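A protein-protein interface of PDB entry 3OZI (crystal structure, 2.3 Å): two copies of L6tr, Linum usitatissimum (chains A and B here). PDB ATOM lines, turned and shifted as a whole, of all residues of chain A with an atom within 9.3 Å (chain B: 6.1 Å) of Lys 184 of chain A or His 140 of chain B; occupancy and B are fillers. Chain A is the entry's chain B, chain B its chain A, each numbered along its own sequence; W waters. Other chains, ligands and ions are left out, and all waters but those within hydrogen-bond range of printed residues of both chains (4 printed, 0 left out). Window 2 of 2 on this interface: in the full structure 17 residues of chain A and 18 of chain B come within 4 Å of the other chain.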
ATOM      1  N   GLN A  50       7.953  31.415  23.276  1.00  0.00           N
ATOM      2  CA  GLN A  50       9.331  31.003  23.034  1.00  0.00           C
ATOM      3  C   GLN A  50       9.589  29.639  23.668  1.00  0.00           C
ATOM      4  O   GLN A  50       8.901  28.659  23.369  1.00  0.00           O
ATOM      5  CB  GLN A  50      10.328  32.033  23.607  1.00  0.00           C
ATOM      6  CG  GLN A  50      10.359  33.417  22.896  1.00  0.00           C
ATOM      7  CD  GLN A  50      10.896  33.346  21.454  1.00  0.00           C
ATOM      8  OE1 GLN A  50      10.111  32.734  20.571  1.00  0.00           O
ATOM      9  NE2 GLN A  50      11.996  33.836  21.140  1.00  0.00           N
ATOM     10  N   PHE A  51      10.567  29.600  24.570  1.00  0.00           N
ATOM     11  CA  PHE A  51      11.012  28.356  25.170  1.00  0.00           C
ATOM     12  C   PHE A  51       9.877  27.504  25.720  1.00  0.00           C
ATOM     13  O   PHE A  51       9.815  26.315  25.460  1.00  0.00           O
ATOM     14  CB  PHE A  51      12.055  28.606  26.264  1.00  0.00           C
ATOM     15  CG  PHE A  51      12.530  27.356  26.917  1.00  0.00           C
ATOM     16  CD1 PHE A  51      13.471  26.557  26.302  1.00  0.00           C
ATOM     17  CD2 PHE A  51      11.990  26.943  28.125  1.00  0.00           C
ATOM     18  CE1 PHE A  51      13.890  25.380  26.898  1.00  0.00           C
ATOM     19  CE2 PHE A  51      12.403  25.776  28.716  1.00  0.00           C
ATOM     20  CZ  PHE A  51      13.356  24.997  28.105  1.00  0.00           C
ATOM     21  N   PHE A  54       8.221  25.714  22.978  1.00  0.00           N
ATOM     22  CA  PHE A  54       9.140  24.708  22.416  1.00  0.00           C
ATOM     23  C   PHE A  54       9.258  23.468  23.325  1.00  0.00           C
ATOM     24  O   PHE A  54       9.244  22.324  22.850  1.00  0.00           O
ATOM     25  CB  PHE A  54      10.530  25.310  22.175  1.00  0.00           C
ATOM     26  CG  PHE A  54      10.532  26.548  21.301  1.00  0.00           C
ATOM     27  CD1 PHE A  54       9.603  26.706  20.282  1.00  0.00           C
ATOM     28  CD2 PHE A  54      11.469  27.550  21.509  1.00  0.00           C
ATOM     29  CE1 PHE A  54       9.607  27.841  19.489  1.00  0.00           C
ATOM     30  CE2 PHE A  54      11.480  28.690  20.720  1.00  0.00           C
ATOM     31  CZ  PHE A  54      10.544  28.838  19.706  1.00  0.00           C
ATOM     32  N   TYR A 131      15.396  31.863  32.416  1.00  0.00           N
ATOM     33  CA  TYR A 131      15.220  32.428  31.095  1.00  0.00           C
ATOM     34  C   TYR A 131      15.678  33.865  31.059  1.00  0.00           C
ATOM     35  O   TYR A 131      14.938  34.764  31.453  1.00  0.00           O
ATOM     36  CB  TYR A 131      13.748  32.348  30.668  1.00  0.00           C
ATOM     37  CG  TYR A 131      13.518  32.762  29.232  1.00  0.00           C
ATOM     38  CD1 TYR A 131      13.640  31.841  28.191  1.00  0.00           C
ATOM     39  CD2 TYR A 131      13.177  34.074  28.910  1.00  0.00           C
ATOM     40  CE1 TYR A 131      13.426  32.212  26.879  1.00  0.00           C
ATOM     41  CE2 TYR A 131      12.965  34.456  27.593  1.00  0.00           C
ATOM     42  CZ  TYR A 131      13.096  33.518  26.585  1.00  0.00           C
ATOM     43  OH  TYR A 131      12.893  33.890  25.278  1.00  0.00           O
ATOM     44  N   MET A 132      16.905  34.075  30.586  1.00  0.00           N
ATOM     45  CA  MET A 132      17.426  35.411  30.312  1.00  0.00           C
ATOM     46  C   MET A 132      17.527  36.263  31.562  1.00  0.00           C
ATOM     47  O   MET A 132      17.445  37.494  31.500  1.00  0.00           O
ATOM     48  CB  MET A 132      16.561  36.117  29.275  1.00  0.00           C
ATOM     49  CG  MET A 132      16.340  35.295  28.031  1.00  0.00           C
ATOM     50  SD  MET A 132      16.982  36.131  26.591  1.00  0.00           S
ATOM     51  CE  MET A 132      16.296  35.140  25.262  1.00  0.00           C
ATOM     52  N   HIS A 178      20.301  27.550  32.269  1.00  0.00           N
ATOM     53  CA  HIS A 178      20.171  28.946  31.920  1.00  0.00           C
ATOM     54  C   HIS A 178      19.905  29.057  30.425  1.00  0.00           C
ATOM     55  O   HIS A 178      20.452  28.289  29.624  1.00  0.00           O
ATOM     56  CB  HIS A 178      21.426  29.728  32.290  1.00  0.00           C
ATOM     57  CG  HIS A 178      21.321  31.190  31.998  1.00  0.00           C
ATOM     58  ND1 HIS A 178      21.842  31.764  30.853  1.00  0.00           N
ATOM     59  CD2 HIS A 178      20.732  32.194  32.691  1.00  0.00           C
ATOM     60  CE1 HIS A 178      21.579  33.059  30.863  1.00  0.00           C
ATOM     61  NE2 HIS A 178      20.911  33.344  31.966  1.00  0.00           N
ATOM     62  N   ILE A 179      19.048  30.001  30.061  1.00  0.00           N
ATOM     63  CA  ILE A 179      18.832  30.338  28.663  1.00  0.00           C
ATOM     64  C   ILE A 179      19.198  31.804  28.442  1.00  0.00           C
ATOM     65  O   ILE A 179      18.683  32.694  29.106  1.00  0.00           O
ATOM     66  CB  ILE A 179      17.394  30.032  28.233  1.00  0.00           C
ATOM     67  CG1 ILE A 179      17.192  28.510  28.225  1.00  0.00           C
ATOM     68  CG2 ILE A 179      17.105  30.627  26.861  1.00  0.00           C
ATOM     69  CD1 ILE A 179      15.888  28.049  27.603  1.00  0.00           C
ATOM     70  N   GLY A 180      20.141  32.047  27.545  1.00  0.00           N
ATOM     71  CA  GLY A 180      20.593  33.400  27.278  1.00  0.00           C
ATOM     72  C   GLY A 180      20.273  33.820  25.857  1.00  0.00           C
ATOM     73  O   GLY A 180      19.671  33.071  25.079  1.00  0.00           O
ATOM     74  N   LYS A 181      20.698  35.022  25.496  1.00  0.00           N
ATOM     75  CA  LYS A 181      20.347  35.563  24.195  1.00  0.00           C
ATOM     76  C   LYS A 181      20.992  34.785  23.038  1.00  0.00           C
ATOM     77  O   LYS A 181      20.482  34.798  21.924  1.00  0.00           O
ATOM     78  CB  LYS A 181      20.671  37.055  24.134  1.00  0.00           C
ATOM     79  CG  LYS A 181      22.145  37.390  24.199  1.00  0.00           C
ATOM     80  CD  LYS A 181      22.344  38.881  23.928  1.00  0.00           C
ATOM     81  CE  LYS A 181      23.822  39.251  23.809  1.00  0.00           C
ATOM     82  NZ  LYS A 181      24.556  39.045  25.092  1.00  0.00           N
ATOM     83  N   ASN A 182      22.082  34.078  23.313  1.00  0.00           N
ATOM     84  CA  ASN A 182      22.794  33.346  22.268  1.00  0.00           C
ATOM     85  C   ASN A 182      22.434  31.871  22.180  1.00  0.00           C
ATOM     86  O   ASN A 182      22.919  31.161  21.306  1.00  0.00           O
ATOM     87  CB  ASN A 182      24.305  33.512  22.441  1.00  0.00           C
ATOM     88  CG  ASN A 182      24.747  34.951  22.237  1.00  0.00           C
ATOM     89  OD1 ASN A 182      24.304  35.609  21.298  1.00  0.00           O
ATOM     90  ND2 ASN A 182      25.598  35.456  23.128  1.00  0.00           N
ATOM     91  N   ASP A 183      21.578  31.409  23.081  1.00  0.00           N
ATOM     92  CA  ASP A 183      21.144  30.028  23.033  1.00  0.00           C
ATOM     93  C   ASP A 183      20.156  29.776  21.916  1.00  0.00           C
ATOM     94  O   ASP A 183      19.344  30.639  21.575  1.00  0.00           O
ATOM     95  CB  ASP A 183      20.561  29.592  24.382  1.00  0.00           C
ATOM     96  CG  ASP A 183      21.624  29.501  25.441  1.00  0.00           C
ATOM     97  OD1 ASP A 183      22.670  28.895  25.139  1.00  0.00           O
ATOM     98  OD2 ASP A 183      21.449  30.064  26.538  1.00  0.00           O
ATOM     99  N   LYS A 184      20.267  28.582  21.344  1.00  0.00           N
ATOM    100  CA  LYS A 184      19.255  28.013  20.469  1.00  0.00           C
ATOM    101  C   LYS A 184      18.223  27.359  21.367  1.00  0.00           C
ATOM    102  O   LYS A 184      18.431  26.237  21.832  1.00  0.00           O
ATOM    103  CB  LYS A 184      19.879  26.949  19.554  1.00  0.00           C
ATOM    104  CG  LYS A 184      20.714  27.489  18.386  1.00  0.00           C
ATOM    105  CD  LYS A 184      21.993  28.202  18.829  1.00  0.00           C
ATOM    106  CE  LYS A 184      22.571  29.118  17.712  1.00  0.00           C
ATOM    107  NZ  LYS A 184      23.394  30.252  18.280  1.00  0.00           N
ATOM    108  N   GLN A 185      17.118  28.051  21.626  1.00  0.00           N
ATOM    109  CA  GLN A 185      16.137  27.566  22.590  1.00  0.00           C
ATOM    110  C   GLN A 185      15.548  26.190  22.232  1.00  0.00           C
ATOM    111  O   GLN A 185      15.207  25.420  23.111  1.00  0.00           O
ATOM    112  CB  GLN A 185      15.043  28.616  22.829  1.00  0.00           C
ATOM    113  CG  GLN A 185      15.613  29.998  23.187  1.00  0.00           C
ATOM    114  CD  GLN A 185      14.556  30.989  23.655  1.00  0.00           C
ATOM    115  OE1 GLN A 185      13.405  30.627  23.918  1.00  0.00           O
ATOM    116  NE2 GLN A 185      14.953  32.250  23.783  1.00  0.00           N
ATOM    117  N   GLY A 186      15.441  25.889  20.944  1.00  0.00           N
ATOM    118  CA  GLY A 186      14.935  24.604  20.494  1.00  0.00           C
ATOM    119  C   GLY A 186      15.845  23.456  20.877  1.00  0.00           C
ATOM    120  O   GLY A 186      15.390  22.355  21.175  1.00  0.00           O
ATOM    121  N   ALA A 187      17.145  23.710  20.873  1.00  0.00           N
ATOM    122  CA  ALA A 187      18.104  22.690  21.257  1.00  0.00           C
ATOM    123  C   ALA A 187      18.015  22.415  22.752  1.00  0.00           C
ATOM    124  O   ALA A 187      18.114  21.268  23.197  1.00  0.00           O
ATOM    125  CB  ALA A 187      19.525  23.104  20.861  1.00  0.00           C
ATOM    126  N   ILE A 188      17.830  23.472  23.533  1.00  0.00           N
ATOM    127  CA  ILE A 188      17.733  23.319  24.972  1.00  0.00           C
ATOM    128  C   ILE A 188      16.467  22.556  25.287  1.00  0.00           C
ATOM    129  O   ILE A 188      16.470  21.624  26.101  1.00  0.00           O
ATOM    130  CB  ILE A 188      17.708  24.678  25.706  1.00  0.00           C
ATOM    131  CG1 ILE A 188      18.899  25.542  25.296  1.00  0.00           C
ATOM    132  CG2 ILE A 188      17.690  24.466  27.201  1.00  0.00           C
ATOM    133  CD1 ILE A 188      20.204  24.794  25.302  1.00  0.00           C
ATOM    134  N   ALA A 189      15.375  22.948  24.633  1.00  0.00           N
ATOM    135  CA  ALA A 189      14.102  22.265  24.823  1.00  0.00           C
ATOM    136  C   ALA A 189      14.255  20.765  24.566  1.00  0.00           C
ATOM    137  O   ALA A 189      13.717  19.947  25.308  1.00  0.00           O
ATOM    138  CB  ALA A 189      13.032  22.865  23.925  1.00  0.00           C
ATOM    139  N   ASP A 190      15.010  20.410  23.526  1.00  0.00           N
ATOM    140  CA  ASP A 190      15.238  19.007  23.189  1.00  0.00           C
ATOM    141  C   ASP A 190      16.044  18.306  24.274  1.00  0.00           C
ATOM    142  O   ASP A 190      15.763  17.160  24.625  1.00  0.00           O
ATOM    143  CB  ASP A 190      15.918  18.868  21.815  1.00  0.00           C
ATOM    144  CG  ASP A 190      14.917  18.898  20.664  1.00  0.00           C
ATOM    145  OD1 ASP A 190      13.711  18.690  20.934  1.00  0.00           O
ATOM    146  OD2 ASP A 190      15.324  19.121  19.495  1.00  0.00           O
ATOM    147  N   LYS A 191      17.037  19.004  24.816  1.00  0.00           N
ATOM    148  CA  LYS A 191      17.860  18.441  25.877  1.00  0.00           C
ATOM    149  C   LYS A 191      17.021  18.253  27.137  1.00  0.00           C
ATOM    150  O   LYS A 191      17.085  17.212  27.787  1.00  0.00           O
ATOM    151  CB  LYS A 191      19.087  19.332  26.157  1.00  0.00           C
ATOM    152  CG  LYS A 191      20.203  19.266  25.080  1.00  0.00           C
ATOM    153  CD  LYS A 191      20.792  17.830  24.933  1.00  0.00           C
ATOM    154  CE  LYS A 191      21.713  17.671  23.687  1.00  0.00           C
ATOM    155  NZ  LYS A 191      23.192  17.937  23.926  1.00  0.00           N
ATOM    156  N   VAL A 192      16.218  19.253  27.471  1.00  0.00           N
ATOM    157  CA  VAL A 192      15.419  19.183  28.676  1.00  0.00           C
ATOM    158  C   VAL A 192      14.370  18.084  28.593  1.00  0.00           C
ATOM    159  O   VAL A 192      14.197  17.318  29.544  1.00  0.00           O
ATOM    160  CB  VAL A 192      14.717  20.508  28.994  1.00  0.00           C
ATOM    161  CG1 VAL A 192      13.743  20.306  30.158  1.00  0.00           C
ATOM    162  CG2 VAL A 192      15.747  21.568  29.346  1.00  0.00           C
ATOM    163  N   PRO B 135      26.752  29.915  29.966  1.00  0.00           N
ATOM    164  CA  PRO B 135      26.572  28.545  29.467  1.00  0.00           C
ATOM    165  C   PRO B 135      26.572  28.480  27.940  1.00  0.00           C
ATOM    166  O   PRO B 135      27.122  27.532  27.388  1.00  0.00           O
ATOM    167  CB  PRO B 135      25.211  28.159  30.043  1.00  0.00           C
ATOM    168  CG  PRO B 135      25.178  28.919  31.373  1.00  0.00           C
ATOM    169  CD  PRO B 135      25.827  30.241  31.066  1.00  0.00           C
ATOM    170  N   SER B 136      25.962  29.474  27.289  1.00  0.00           N
ATOM    171  CA  SER B 136      26.024  29.681  25.842  1.00  0.00           C
ATOM    172  C   SER B 136      27.405  29.418  25.277  1.00  0.00           C
ATOM    173  O   SER B 136      27.571  28.658  24.322  1.00  0.00           O
ATOM    174  CB  SER B 136      25.694  31.138  25.519  1.00  0.00           C
ATOM    175  OG  SER B 136      24.389  31.260  25.028  1.00  0.00           O
ATOM    176  N   ASP B 137      28.392  30.092  25.850  1.00  0.00           N
ATOM    177  CA  ASP B 137      29.780  29.952  25.404  1.00  0.00           C
ATOM    178  C   ASP B 137      30.341  28.545  25.586  1.00  0.00           C
ATOM    179  O   ASP B 137      31.060  28.056  24.716  1.00  0.00           O
ATOM    180  CB  ASP B 137      30.683  30.985  26.080  1.00  0.00           C
ATOM    181  CG  ASP B 137      30.459  32.377  25.535  1.00  0.00           C
ATOM    182  OD1 ASP B 137      29.985  32.481  24.393  1.00  0.00           O
ATOM    183  OD2 ASP B 137      30.750  33.361  26.237  1.00  0.00           O
ATOM    184  N   VAL B 138      30.029  27.892  26.706  1.00  0.00           N
ATOM    185  CA  VAL B 138      30.501  26.516  26.880  1.00  0.00           C
ATOM    186  C   VAL B 138      29.857  25.650  25.809  1.00  0.00           C
ATOM    187  O   VAL B 138      30.525  24.888  25.120  1.00  0.00           O
ATOM    188  CB  VAL B 138      30.182  25.951  28.283  1.00  0.00           C
ATOM    189  CG1 VAL B 138      30.581  24.456  28.382  1.00  0.00           C
ATOM    190  CG2 VAL B 138      30.857  26.798  29.377  1.00  0.00           C
ATOM    191  N   ARG B 139      28.550  25.808  25.662  1.00  0.00           N
ATOM    192  CA  ARG B 139      27.757  25.037  24.710  1.00  0.00           C
ATOM    193  C   ARG B 139      28.230  25.153  23.262  1.00  0.00           C
ATOM    194  O   ARG B 139      28.165  24.179  22.512  1.00  0.00           O
ATOM    195  CB  ARG B 139      26.285  25.464  24.793  1.00  0.00           C
ATOM    196  CG  ARG B 139      25.539  24.979  26.045  1.00  0.00           C
ATOM    197  CD  ARG B 139      24.287  25.827  26.283  1.00  0.00           C
ATOM    198  NE  ARG B 139      23.613  25.469  27.529  1.00  0.00           N
ATOM    199  CZ  ARG B 139      22.693  26.228  28.114  1.00  0.00           C
ATOM    200  NH1 ARG B 139      22.334  27.388  27.563  1.00  0.00           N
ATOM    201  NH2 ARG B 139      22.131  25.831  29.248  1.00  0.00           N
ATOM    202  N   HIS B 140      28.686  26.343  22.867  1.00  0.00           N
ATOM    203  CA  HIS B 140      29.064  26.593  21.471  1.00  0.00           C
ATOM    204  C   HIS B 140      30.553  26.882  21.330  1.00  0.00           C
ATOM    205  O   HIS B 140      31.044  27.122  20.233  1.00  0.00           O
ATOM    206  CB  HIS B 140      28.241  27.745  20.882  1.00  0.00           C
ATOM    207  CG  HIS B 140      26.762  27.546  21.015  1.00  0.00           C
ATOM    208  ND1 HIS B 140      25.929  28.487  21.583  1.00  0.00           N
ATOM    209  CD2 HIS B 140      25.969  26.501  20.676  1.00  0.00           C
ATOM    210  CE1 HIS B 140      24.688  28.036  21.579  1.00  0.00           C
ATOM    211  NE2 HIS B 140      24.685  26.831  21.039  1.00  0.00           N
ATOM    212  N   GLN B 141      31.268  26.843  22.448  1.00  0.00           N
ATOM    213  CA  GLN B 141      32.707  27.077  22.427  1.00  0.00           C
ATOM    214  C   GLN B 141      32.979  28.414  21.759  1.00  0.00           C
ATOM    215  O   GLN B 141      33.819  28.514  20.870  1.00  0.00           O
ATOM    216  CB  GLN B 141      33.430  25.945  21.679  1.00  0.00           C
ATOM    217  CG  GLN B 141      33.232  24.554  22.301  1.00  0.00           C
ATOM    218  CD  GLN B 141      32.005  23.824  21.759  1.00  0.00           C
ATOM    219  OE1 GLN B 141      31.943  23.498  20.573  1.00  0.00           O
ATOM    220  NE2 GLN B 141      31.029  23.547  22.635  1.00  0.00           N
ATOM    221  N   THR B 142      32.229  29.430  22.172  1.00  0.00           N
ATOM    222  CA  THR B 142      32.422  30.784  21.665  1.00  0.00           C
ATOM    223  C   THR B 142      33.044  31.630  22.762  1.00  0.00           C
ATOM    224  O   THR B 142      33.455  31.098  23.804  1.00  0.00           O
ATOM    225  CB  THR B 142      31.097  31.428  21.188  1.00  0.00           C
ATOM    226  OG1 THR B 142      30.136  31.432  22.258  1.00  0.00           O
ATOM    227  CG2 THR B 142      30.535  30.662  19.994  1.00  0.00           C
ATOM    228  N   LYS B 146      37.029  30.475  22.020  1.00  0.00           N
ATOM    229  CA  LYS B 146      37.449  30.529  20.616  1.00  0.00           C
ATOM    230  C   LYS B 146      38.955  30.364  20.457  1.00  0.00           C
ATOM    231  O   LYS B 146      39.436  29.442  19.781  1.00  0.00           O
ATOM    232  CB  LYS B 146      37.034  31.857  19.976  1.00  0.00           C
ATOM    233  CG  LYS B 146      35.608  31.896  19.460  1.00  0.00           C
ATOM    234  CD  LYS B 146      35.377  30.837  18.404  1.00  0.00           C
ATOM    235  CE  LYS B 146      33.976  30.950  17.818  1.00  0.00           C
ATOM    236  NZ  LYS B 146      33.624  29.735  17.019  1.00  0.00           N
ATOM    237  N   LYS B 165      35.301  19.567  21.478  1.00  0.00           N
ATOM    238  CA  LYS B 165      34.169  20.478  21.343  1.00  0.00           C
ATOM    239  C   LYS B 165      32.858  19.787  21.710  1.00  0.00           C
ATOM    240  O   LYS B 165      32.016  20.368  22.392  1.00  0.00           O
ATOM    241  CB  LYS B 165      34.088  21.053  19.927  1.00  0.00           C
ATOM    242  CG  LYS B 165      35.222  22.021  19.588  1.00  0.00           C
ATOM    243  CD  LYS B 165      34.953  22.725  18.273  1.00  0.00           C
ATOM    244  CE  LYS B 165      35.844  23.951  18.126  1.00  0.00           C
ATOM    245  NZ  LYS B 165      35.433  24.786  16.959  1.00  0.00           N
ATOM    246  N   LYS B 169      30.038  20.715  24.551  1.00  0.00           N
ATOM    247  CA  LYS B 169      28.650  20.901  24.157  1.00  0.00           C
ATOM    248  C   LYS B 169      27.726  19.976  24.958  1.00  0.00           C
ATOM    249  O   LYS B 169      26.730  20.422  25.543  1.00  0.00           O
ATOM    250  CB  LYS B 169      28.458  20.665  22.657  1.00  0.00           C
ATOM    251  CG  LYS B 169      27.038  21.001  22.205  1.00  0.00           C
ATOM    252  CD  LYS B 169      26.691  20.362  20.865  1.00  0.00           C
ATOM    253  CE  LYS B 169      25.930  21.340  19.980  1.00  0.00           C
ATOM    254  NZ  LYS B 169      25.407  20.671  18.749  1.00  0.00           N
HETATM  255  O   HOH W   1      23.874  33.881  25.814  1.00  0.00           O
HETATM  256  O   HOH W   2      22.102  27.106  23.125  1.00  0.00           O
HETATM  257  O   HOH W   3      22.730  26.388  32.517  1.00  0.00           O
HETATM  258  O   HOH W   4      23.094  30.832  28.597  1.00  0.00           O
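A ring nitrogen (ND1) of His 140 of chain B is in hydrogen-bond range of the backbone carbonyl oxygen (O) of Ser 136 of chain B (3.2 Å).
The backbone carbonyl oxygen of Arg 139 of chain B lies within hydrogen-bond range of the side-chain amide nitrogen of Gln 141 of chain B.
The side-chain carboxylate (OD2) of Asp 183 of chain A lies within hydrogen-bond range of the backbone NH (N) of Gly 180 of chain A, at 2.6 Å.
The backbone carbonyl oxygen (O) of Asn 182 of chain A is in hydrogen-bond range of the side-chain amino group (NZ) of Lys 184 of chain A, 3.2 Å away.
No position is printed for both chains.
Water W3 lies within hydrogen-bond range of N of His 178 of chain A (2.7 Å) and NH2 of Arg 139 of chain B (3.4 Å).
Water W4 lies within hydrogen-bond range of ND1 of His 178 of chain A, OD2 of Asp 183 of chain A, N of Gly 180 of chain A and N of Ser 136 of chain B.
Water W2 lies within hydrogen-bond range of OD1 of Asp 183 of chain A (2.8 Å), N of Lys 184 of chain A (3.0 Å) and NE2 of His 140 of chain B (3.3 Å).
Water W1 lies within hydrogen-bond range of OG of Ser 136 of chain B (2.8 Å), N of Asn 182 of chain A (3.1 Å) and N of Lys 181 of chain A (3.4 Å).
OD1 of Asp 183 of chain A is in salt-bridge range of NH1 of Arg 139 of chain B (2.9 Å).
The guanidinium group of Arg 139 of chain B sits at hydrogen-bond distance from the backbone carbonyl oxygen of His 178 of chain A (2.9 Å).
The side-chain carboxylate (OD1) of Asp 183 of chain A is in hydrogen-bond range of the side-chain hydroxyl (OG) of Ser 136 of chain B, 2.9 Å away.
Hydrophobic or aromatic side chains of chain A within 4 Å of the printed part of chain B: His 178.
Among the printed residues, 7 pairs touch across the chains.
Among the printed residues, Asp or Glu carboxylates within 4 Å of a Lys or Arg side-chain nitrogen of the other chain: Asp 183 of chain A with Arg 139 of chain B.
Met 132 of chain A touches none of the printed residues of chain B.
Printed residues of chain B within 4 Å of His 178 of chain A: Pro 135 and Arg 139.
Of the printed residues of chain B, Asp 183 of chain A touches Ser 136 (2.9 Å) and Arg 139 (2.9 Å).
Of chain B, only His 140 comes within 4 Å of Lys 184 of chain A.
Of the printed residues of chain A, Pro 135 of chain B touches His 178 (3.9 Å).
Printed residues of chain A within 4 Å of Ser 136 of chain B: Asn 182 and Asp 183.
Of the printed residues of chain A, Arg 139 of chain B touches His 178 and Asp 183.
His 140 of chain B touches just these residues of chain A: Asn 182 and Lys 184.
The nearest printed residue of chain B that does not touch Lys 184 of chain A is Ser 136 of chain B (6.1 Å).
The nearest printed residue of chain A that does not touch Pro 135 of chain B is Asp 183 of chain A (4.8 Å).
His 178 of chain A touches Pro 135 of chain B (CB to CG, 3.9 Å).
Ser 136 of chain B touches Asn 182 of chain A.
Asn 182 of chain A touches His 140 of chain B (O to CE1, 3.6 Å).
CD of Lys 184 of chain A touches NE2 of His 140 of chain B, at 3.7 Å.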
